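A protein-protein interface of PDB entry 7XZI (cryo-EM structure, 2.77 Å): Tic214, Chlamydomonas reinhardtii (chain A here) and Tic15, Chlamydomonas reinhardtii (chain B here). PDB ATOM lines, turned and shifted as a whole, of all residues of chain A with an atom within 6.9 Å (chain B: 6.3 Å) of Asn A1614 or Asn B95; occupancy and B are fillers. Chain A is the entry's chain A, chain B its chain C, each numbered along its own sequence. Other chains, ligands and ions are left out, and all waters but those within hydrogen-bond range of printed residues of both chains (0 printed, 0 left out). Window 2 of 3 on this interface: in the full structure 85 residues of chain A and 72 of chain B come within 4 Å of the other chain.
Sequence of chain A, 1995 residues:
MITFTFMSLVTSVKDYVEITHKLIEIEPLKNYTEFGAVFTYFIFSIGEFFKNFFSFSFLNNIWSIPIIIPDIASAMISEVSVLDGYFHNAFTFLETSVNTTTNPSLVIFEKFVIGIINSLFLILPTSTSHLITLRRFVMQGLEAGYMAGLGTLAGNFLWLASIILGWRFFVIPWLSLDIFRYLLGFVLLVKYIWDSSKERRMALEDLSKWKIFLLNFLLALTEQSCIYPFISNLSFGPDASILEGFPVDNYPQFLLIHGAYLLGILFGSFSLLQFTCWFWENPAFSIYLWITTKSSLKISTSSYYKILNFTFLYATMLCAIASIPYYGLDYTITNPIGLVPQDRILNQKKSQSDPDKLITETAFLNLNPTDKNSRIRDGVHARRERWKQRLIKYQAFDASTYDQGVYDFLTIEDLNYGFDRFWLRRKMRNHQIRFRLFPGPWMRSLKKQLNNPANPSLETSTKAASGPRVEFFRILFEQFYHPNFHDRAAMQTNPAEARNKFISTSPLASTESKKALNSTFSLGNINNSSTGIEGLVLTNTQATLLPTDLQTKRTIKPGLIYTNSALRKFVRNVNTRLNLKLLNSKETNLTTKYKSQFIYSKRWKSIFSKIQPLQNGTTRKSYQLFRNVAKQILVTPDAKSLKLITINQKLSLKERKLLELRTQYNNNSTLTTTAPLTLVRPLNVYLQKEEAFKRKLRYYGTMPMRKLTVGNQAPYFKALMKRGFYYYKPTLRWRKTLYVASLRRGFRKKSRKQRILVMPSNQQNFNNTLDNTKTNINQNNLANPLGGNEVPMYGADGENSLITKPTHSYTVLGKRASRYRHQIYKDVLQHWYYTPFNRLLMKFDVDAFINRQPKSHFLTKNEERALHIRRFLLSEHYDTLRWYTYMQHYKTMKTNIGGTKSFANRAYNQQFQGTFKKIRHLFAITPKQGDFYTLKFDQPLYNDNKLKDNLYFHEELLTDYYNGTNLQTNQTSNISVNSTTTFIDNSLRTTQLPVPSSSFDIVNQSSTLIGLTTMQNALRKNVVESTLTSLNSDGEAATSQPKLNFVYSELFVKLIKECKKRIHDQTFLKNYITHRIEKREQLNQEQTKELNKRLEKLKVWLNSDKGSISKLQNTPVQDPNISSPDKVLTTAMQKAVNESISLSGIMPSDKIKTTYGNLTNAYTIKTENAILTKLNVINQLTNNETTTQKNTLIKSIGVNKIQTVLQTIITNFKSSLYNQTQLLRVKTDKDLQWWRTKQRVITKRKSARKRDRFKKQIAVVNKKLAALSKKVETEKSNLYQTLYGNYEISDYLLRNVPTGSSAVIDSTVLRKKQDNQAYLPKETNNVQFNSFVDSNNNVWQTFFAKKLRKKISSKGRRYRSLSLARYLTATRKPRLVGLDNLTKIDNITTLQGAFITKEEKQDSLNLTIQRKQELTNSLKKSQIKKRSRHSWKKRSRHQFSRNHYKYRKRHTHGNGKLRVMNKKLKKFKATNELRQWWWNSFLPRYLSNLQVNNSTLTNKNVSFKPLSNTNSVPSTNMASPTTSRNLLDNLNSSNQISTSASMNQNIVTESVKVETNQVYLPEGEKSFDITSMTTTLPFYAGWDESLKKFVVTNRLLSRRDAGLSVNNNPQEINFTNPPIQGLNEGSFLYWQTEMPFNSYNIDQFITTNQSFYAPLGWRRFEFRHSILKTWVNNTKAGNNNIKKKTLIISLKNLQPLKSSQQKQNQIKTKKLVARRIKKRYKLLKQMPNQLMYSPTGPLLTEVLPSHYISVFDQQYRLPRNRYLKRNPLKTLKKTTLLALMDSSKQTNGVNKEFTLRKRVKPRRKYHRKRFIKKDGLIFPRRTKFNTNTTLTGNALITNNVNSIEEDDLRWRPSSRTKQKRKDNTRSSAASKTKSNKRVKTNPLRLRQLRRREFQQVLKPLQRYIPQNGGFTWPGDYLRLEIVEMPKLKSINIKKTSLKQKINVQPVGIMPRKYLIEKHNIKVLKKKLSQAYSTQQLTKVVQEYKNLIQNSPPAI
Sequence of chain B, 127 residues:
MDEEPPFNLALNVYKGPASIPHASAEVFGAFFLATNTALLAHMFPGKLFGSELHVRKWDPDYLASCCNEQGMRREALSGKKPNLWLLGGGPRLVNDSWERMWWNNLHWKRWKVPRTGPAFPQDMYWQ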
ATOM      1  N   LEU A1604      22.910   5.660 -22.327  1.00  0.00           N
ATOM      2  CA  LEU A1604      22.583   4.239 -22.328  1.00  0.00           C
ATOM      3  C   LEU A1604      22.484   3.686 -23.745  1.00  0.00           C
ATOM      4  O   LEU A1604      22.898   2.549 -24.002  1.00  0.00           O
ATOM      5  CB  LEU A1604      21.278   3.998 -21.570  1.00  0.00           C
ATOM      6  CG  LEU A1604      21.291   4.331 -20.079  1.00  0.00           C
ATOM      7  CD1 LEU A1604      19.976   3.940 -19.424  1.00  0.00           C
ATOM      8  CD2 LEU A1604      22.459   3.644 -19.392  1.00  0.00           C
ATOM      9  N   SER A1605      21.938   4.465 -24.674  1.00  0.00           N
ATOM     10  CA  SER A1605      21.718   3.984 -26.032  1.00  0.00           C
ATOM     11  C   SER A1605      21.673   5.172 -26.981  1.00  0.00           C
ATOM     12  O   SER A1605      21.513   6.321 -26.564  1.00  0.00           O
ATOM     13  CB  SER A1605      20.431   3.160 -26.129  1.00  0.00           C
ATOM     14  OG  SER A1605      19.300   3.945 -25.796  1.00  0.00           O
ATOM     15  N   VAL A1606      21.816   4.875 -28.271  1.00  0.00           N
ATOM     16  CA  VAL A1606      21.726   5.869 -29.333  1.00  0.00           C
ATOM     17  C   VAL A1606      20.826   5.325 -30.431  1.00  0.00           C
ATOM     18  O   VAL A1606      20.721   4.108 -30.617  1.00  0.00           O
ATOM     19  CB  VAL A1606      23.111   6.233 -29.906  1.00  0.00           C
ATOM     20  CG1 VAL A1606      23.963   6.922 -28.850  1.00  0.00           C
ATOM     21  CG2 VAL A1606      23.808   4.993 -30.440  1.00  0.00           C
ATOM     22  N   GLU A1612      17.908   0.874 -33.105  1.00  0.00           N
ATOM     23  CA  GLU A1612      18.515   1.357 -31.874  1.00  0.00           C
ATOM     24  C   GLU A1612      19.689   0.472 -31.465  1.00  0.00           C
ATOM     25  O   GLU A1612      19.669  -0.748 -31.639  1.00  0.00           O
ATOM     26  CB  GLU A1612      17.472   1.411 -30.757  1.00  0.00           C
ATOM     27  CG  GLU A1612      17.968   2.036 -29.467  1.00  0.00           C
ATOM     28  CD  GLU A1612      16.840   2.365 -28.511  1.00  0.00           C
ATOM     29  OE1 GLU A1612      15.687   2.491 -28.973  1.00  0.00           O
ATOM     30  OE2 GLU A1612      17.108   2.496 -27.298  1.00  0.00           O
ATOM     31  N   ILE A1613      20.721   1.107 -30.914  1.00  0.00           N
ATOM     32  CA  ILE A1613      21.939   0.429 -30.479  1.00  0.00           C
ATOM     33  C   ILE A1613      22.092   0.651 -28.980  1.00  0.00           C
ATOM     34  O   ILE A1613      22.099   1.796 -28.515  1.00  0.00           O
ATOM     35  CB  ILE A1613      23.179   0.941 -31.230  1.00  0.00           C
ATOM     36  CG1 ILE A1613      23.063   0.660 -32.730  1.00  0.00           C
ATOM     37  CG2 ILE A1613      24.445   0.320 -30.659  1.00  0.00           C
ATOM     38  CD1 ILE A1613      24.243   1.164 -33.536  1.00  0.00           C
ATOM     39  N   ASN A1614      22.224  -0.441 -28.227  1.00  0.00           N
ATOM     40  CA  ASN A1614      22.429  -0.383 -26.786  1.00  0.00           C
ATOM     41  C   ASN A1614      23.895  -0.642 -26.455  1.00  0.00           C
ATOM     42  O   ASN A1614      24.503  -1.579 -26.978  1.00  0.00           O
ATOM     43  CB  ASN A1614      21.545  -1.401 -26.061  1.00  0.00           C
ATOM     44  CG  ASN A1614      20.060  -1.089 -26.184  1.00  0.00           C
ATOM     45  OD1 ASN A1614      19.637  -0.345 -27.067  1.00  0.00           O
ATOM     46  ND2 ASN A1614      19.262  -1.667 -25.293  1.00  0.00           N
ATOM     47  N   PHE A1615      24.456   0.192 -25.580  1.00  0.00           N
ATOM     48  CA  PHE A1615      25.869   0.142 -25.215  1.00  0.00           C
ATOM     49  C   PHE A1615      26.034  -0.809 -24.032  1.00  0.00           C
ATOM     50  O   PHE A1615      25.302  -0.709 -23.044  1.00  0.00           O
ATOM     51  CB  PHE A1615      26.383   1.541 -24.877  1.00  0.00           C
ATOM     52  CG  PHE A1615      26.369   2.497 -26.041  1.00  0.00           C
ATOM     53  CD1 PHE A1615      26.718   2.069 -27.308  1.00  0.00           C
ATOM     54  CD2 PHE A1615      26.008   3.823 -25.865  1.00  0.00           C
ATOM     55  CE1 PHE A1615      26.712   2.942 -28.377  1.00  0.00           C
ATOM     56  CE2 PHE A1615      25.998   4.700 -26.934  1.00  0.00           C
ATOM     57  CZ  PHE A1615      26.353   4.259 -28.189  1.00  0.00           C
ATOM     58  N   THR A1616      26.983  -1.741 -24.130  1.00  0.00           N
ATOM     59  CA  THR A1616      27.135  -2.713 -23.053  1.00  0.00           C
ATOM     60  C   THR A1616      28.184  -2.267 -22.040  1.00  0.00           C
ATOM     61  O   THR A1616      27.871  -2.092 -20.855  1.00  0.00           O
ATOM     62  CB  THR A1616      27.490  -4.084 -23.627  1.00  0.00           C
ATOM     63  OG1 THR A1616      28.817  -4.057 -24.165  1.00  0.00           O
ATOM     64  CG2 THR A1616      26.515  -4.452 -24.734  1.00  0.00           C
ATOM     65  N   ASN A1617      29.426  -2.061 -22.492  1.00  0.00           N
ATOM     66  CA  ASN A1617      30.562  -1.841 -21.610  1.00  0.00           C
ATOM     67  C   ASN A1617      30.464  -0.504 -20.878  1.00  0.00           C
ATOM     68  O   ASN A1617      30.818  -0.419 -19.699  1.00  0.00           O
ATOM     69  CB  ASN A1617      31.876  -1.872 -22.399  1.00  0.00           C
ATOM     70  CG  ASN A1617      32.145  -3.226 -23.027  1.00  0.00           C
ATOM     71  OD1 ASN A1617      31.229  -4.026 -23.249  1.00  0.00           O
ATOM     72  ND2 ASN A1617      33.406  -3.491 -23.334  1.00  0.00           N
ATOM     73  N   PRO A1618      29.947   0.544 -21.528  1.00  0.00           N
ATOM     74  CA  PRO A1618      30.173   1.915 -21.055  1.00  0.00           C
ATOM     75  C   PRO A1618      29.735   2.084 -19.611  1.00  0.00           C
ATOM     76  O   PRO A1618      30.556   2.408 -18.740  1.00  0.00           O
ATOM     77  N   ARG B  92      32.016   6.726 -34.939  1.00  0.00           N
ATOM     78  CA  ARG B  92      32.498   5.382 -35.230  1.00  0.00           C
ATOM     79  C   ARG B  92      31.397   4.380 -34.921  1.00  0.00           C
ATOM     80  O   ARG B  92      30.824   4.402 -33.828  1.00  0.00           O
ATOM     81  CB  ARG B  92      33.748   5.052 -34.414  1.00  0.00           C
ATOM     82  CG  ARG B  92      34.913   5.988 -34.651  1.00  0.00           C
ATOM     83  CD  ARG B  92      36.093   5.611 -33.777  1.00  0.00           C
ATOM     84  NE  ARG B  92      37.217   6.514 -33.965  1.00  0.00           N
ATOM     85  CZ  ARG B  92      38.364   6.428 -33.302  1.00  0.00           C
ATOM     86  NH1 ARG B  92      38.567   5.488 -32.394  1.00  0.00           N
ATOM     87  NH2 ARG B  92      39.328   7.307 -33.557  1.00  0.00           N
ATOM     88  N   LEU B  93      31.109   3.502 -35.877  1.00  0.00           N
ATOM     89  CA  LEU B  93      30.041   2.521 -35.714  1.00  0.00           C
ATOM     90  C   LEU B  93      30.498   1.438 -34.744  1.00  0.00           C
ATOM     91  O   LEU B  93      31.116   0.449 -35.141  1.00  0.00           O
ATOM     92  CB  LEU B  93      29.656   1.927 -37.064  1.00  0.00           C
ATOM     93  CG  LEU B  93      28.508   0.917 -37.041  1.00  0.00           C
ATOM     94  CD1 LEU B  93      27.278   1.530 -36.396  1.00  0.00           C
ATOM     95  CD2 LEU B  93      28.193   0.429 -38.445  1.00  0.00           C
ATOM     96  N   VAL B  94      30.193   1.624 -33.460  1.00  0.00           N
ATOM     97  CA  VAL B  94      30.514   0.659 -32.418  1.00  0.00           C
ATOM     98  C   VAL B  94      29.281   0.461 -31.550  1.00  0.00           C
ATOM     99  O   VAL B  94      28.369   1.294 -31.535  1.00  0.00           O
ATOM    100  CB  VAL B  94      31.713   1.110 -31.554  1.00  0.00           C
ATOM    101  CG1 VAL B  94      32.976   1.188 -32.394  1.00  0.00           C
ATOM    102  CG2 VAL B  94      31.416   2.449 -30.897  1.00  0.00           C
ATOM    103  N   ASN B  95      29.256  -0.654 -30.822  1.00  0.00           N
ATOM    104  CA  ASN B  95      28.144  -0.979 -29.941  1.00  0.00           C
ATOM    105  C   ASN B  95      28.534  -0.999 -28.470  1.00  0.00           C
ATOM    106  O   ASN B  95      27.708  -1.375 -27.630  1.00  0.00           O
ATOM    107  CB  ASN B  95      27.531  -2.329 -30.332  1.00  0.00           C
ATOM    108  CG  ASN B  95      28.507  -3.480 -30.193  1.00  0.00           C
ATOM    109  OD1 ASN B  95      29.717  -3.304 -30.337  1.00  0.00           O
ATOM    110  ND2 ASN B  95      27.984  -4.669 -29.918  1.00  0.00           N
ATOM    111  N   ASP B  96      29.759  -0.607 -28.134  1.00  0.00           N
ATOM    112  CA  ASP B  96      30.241  -0.579 -26.755  1.00  0.00           C
ATOM    113  C   ASP B  96      30.574   0.863 -26.389  1.00  0.00           C
ATOM    114  O   ASP B  96      31.447   1.483 -27.005  1.00  0.00           O
ATOM    115  CB  ASP B  96      31.449  -1.498 -26.582  1.00  0.00           C
ATOM    116  CG  ASP B  96      32.557  -1.202 -27.576  1.00  0.00           C
ATOM    117  OD1 ASP B  96      32.244  -0.829 -28.726  1.00  0.00           O
ATOM    118  OD2 ASP B  96      33.742  -1.342 -27.207  1.00  0.00           O
ATOM    119  N   SER B  97      29.844   1.402 -25.409  1.00  0.00           N
ATOM    120  CA  SER B  97      30.085   2.719 -24.823  1.00  0.00           C
ATOM    121  C   SER B  97      29.726   3.851 -25.779  1.00  0.00           C
ATOM    122  O   SER B  97      29.759   3.685 -27.003  1.00  0.00           O
ATOM    123  CB  SER B  97      31.541   2.867 -24.369  1.00  0.00           C
ATOM    124  OG  SER B  97      32.416   3.013 -25.473  1.00  0.00           O
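Among the printed residues, merely in contact across the chains: Ile A1613 with Asn B95, Phe A1615 with Val B94, Phe A1615 with Asn B95, Phe A1615 with Ser B97, Thr A1616 with Asn B95 and Pro A1618 with Ser B97.
Along chain B the printed residues that touch a printed residue of chain A span positions 94 to 97.
Of the 10 printed residues of chain A, 5 touch a printed residue of chain B.
Hydrophobic or aromatic side chains of chain A within 4 Å of the printed part of chain B: Ile A1613 and Phe A1615.
Among the printed residues, 7 pairs touch across the chains.
Among the printed residues, no Asp or Glu carboxylate lies within 4 Å of a Lys or Arg side-chain nitrogen of the other chain.
Of chain B, only Asn B95 (3.3 Å) comes within 4 Å of Asn A1614.
Printed residues of chain A within 4 Å of Asn B95: Ile A1613 (3.99 Å), Asn A1614 (3.3 Å), Phe A1615 (3.4 Å) and Thr A1616 (3.6 Å).
Of the printed residues of chain B, Phe A1615 touches Val B94, Asn B95 and Ser B97.
Printed residues of chain B within 4 Å of Pro A1618: Ser B97 (3.7 Å).
Of the printed residues of chain B, Thr A1616 touches Asn B95 (3.6 Å).
Asp B96 touches none of the printed residues of chain A.
Arg B92 touches none of the printed residues of chain A.
The nearest residue of chain B that does not touch Asn A1614 is Asp B96 (5.5 Å).
The nearest printed residue of chain A that does not touch Asn B95 is Asn A1617 (5.5 Å).
The nearest printed residue of chain A that does not touch Val B94 is Ile A1613 (4.1 Å).
The backbone carbonyl oxygen (O) of Asn A1614 sits close to the backbone carbonyl oxygen (O) of Asn B95, at 3.3 Å.
The side-chain amide oxygen (OD1) of Asn A1617 is in hydrogen-bond range of the side-chain hydroxyl (OG1) of Thr A1616.
The backbone carbonyl oxygen (O) of Leu A1604 lies within hydrogen-bond range of the backbone NH (N) of Phe A1615 (3.2 Å).
The backbone NH (N) of Ile A1613 lies within hydrogen-bond range of the backbone carbonyl oxygen (O) of Val A1606, at 3.0 Å.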
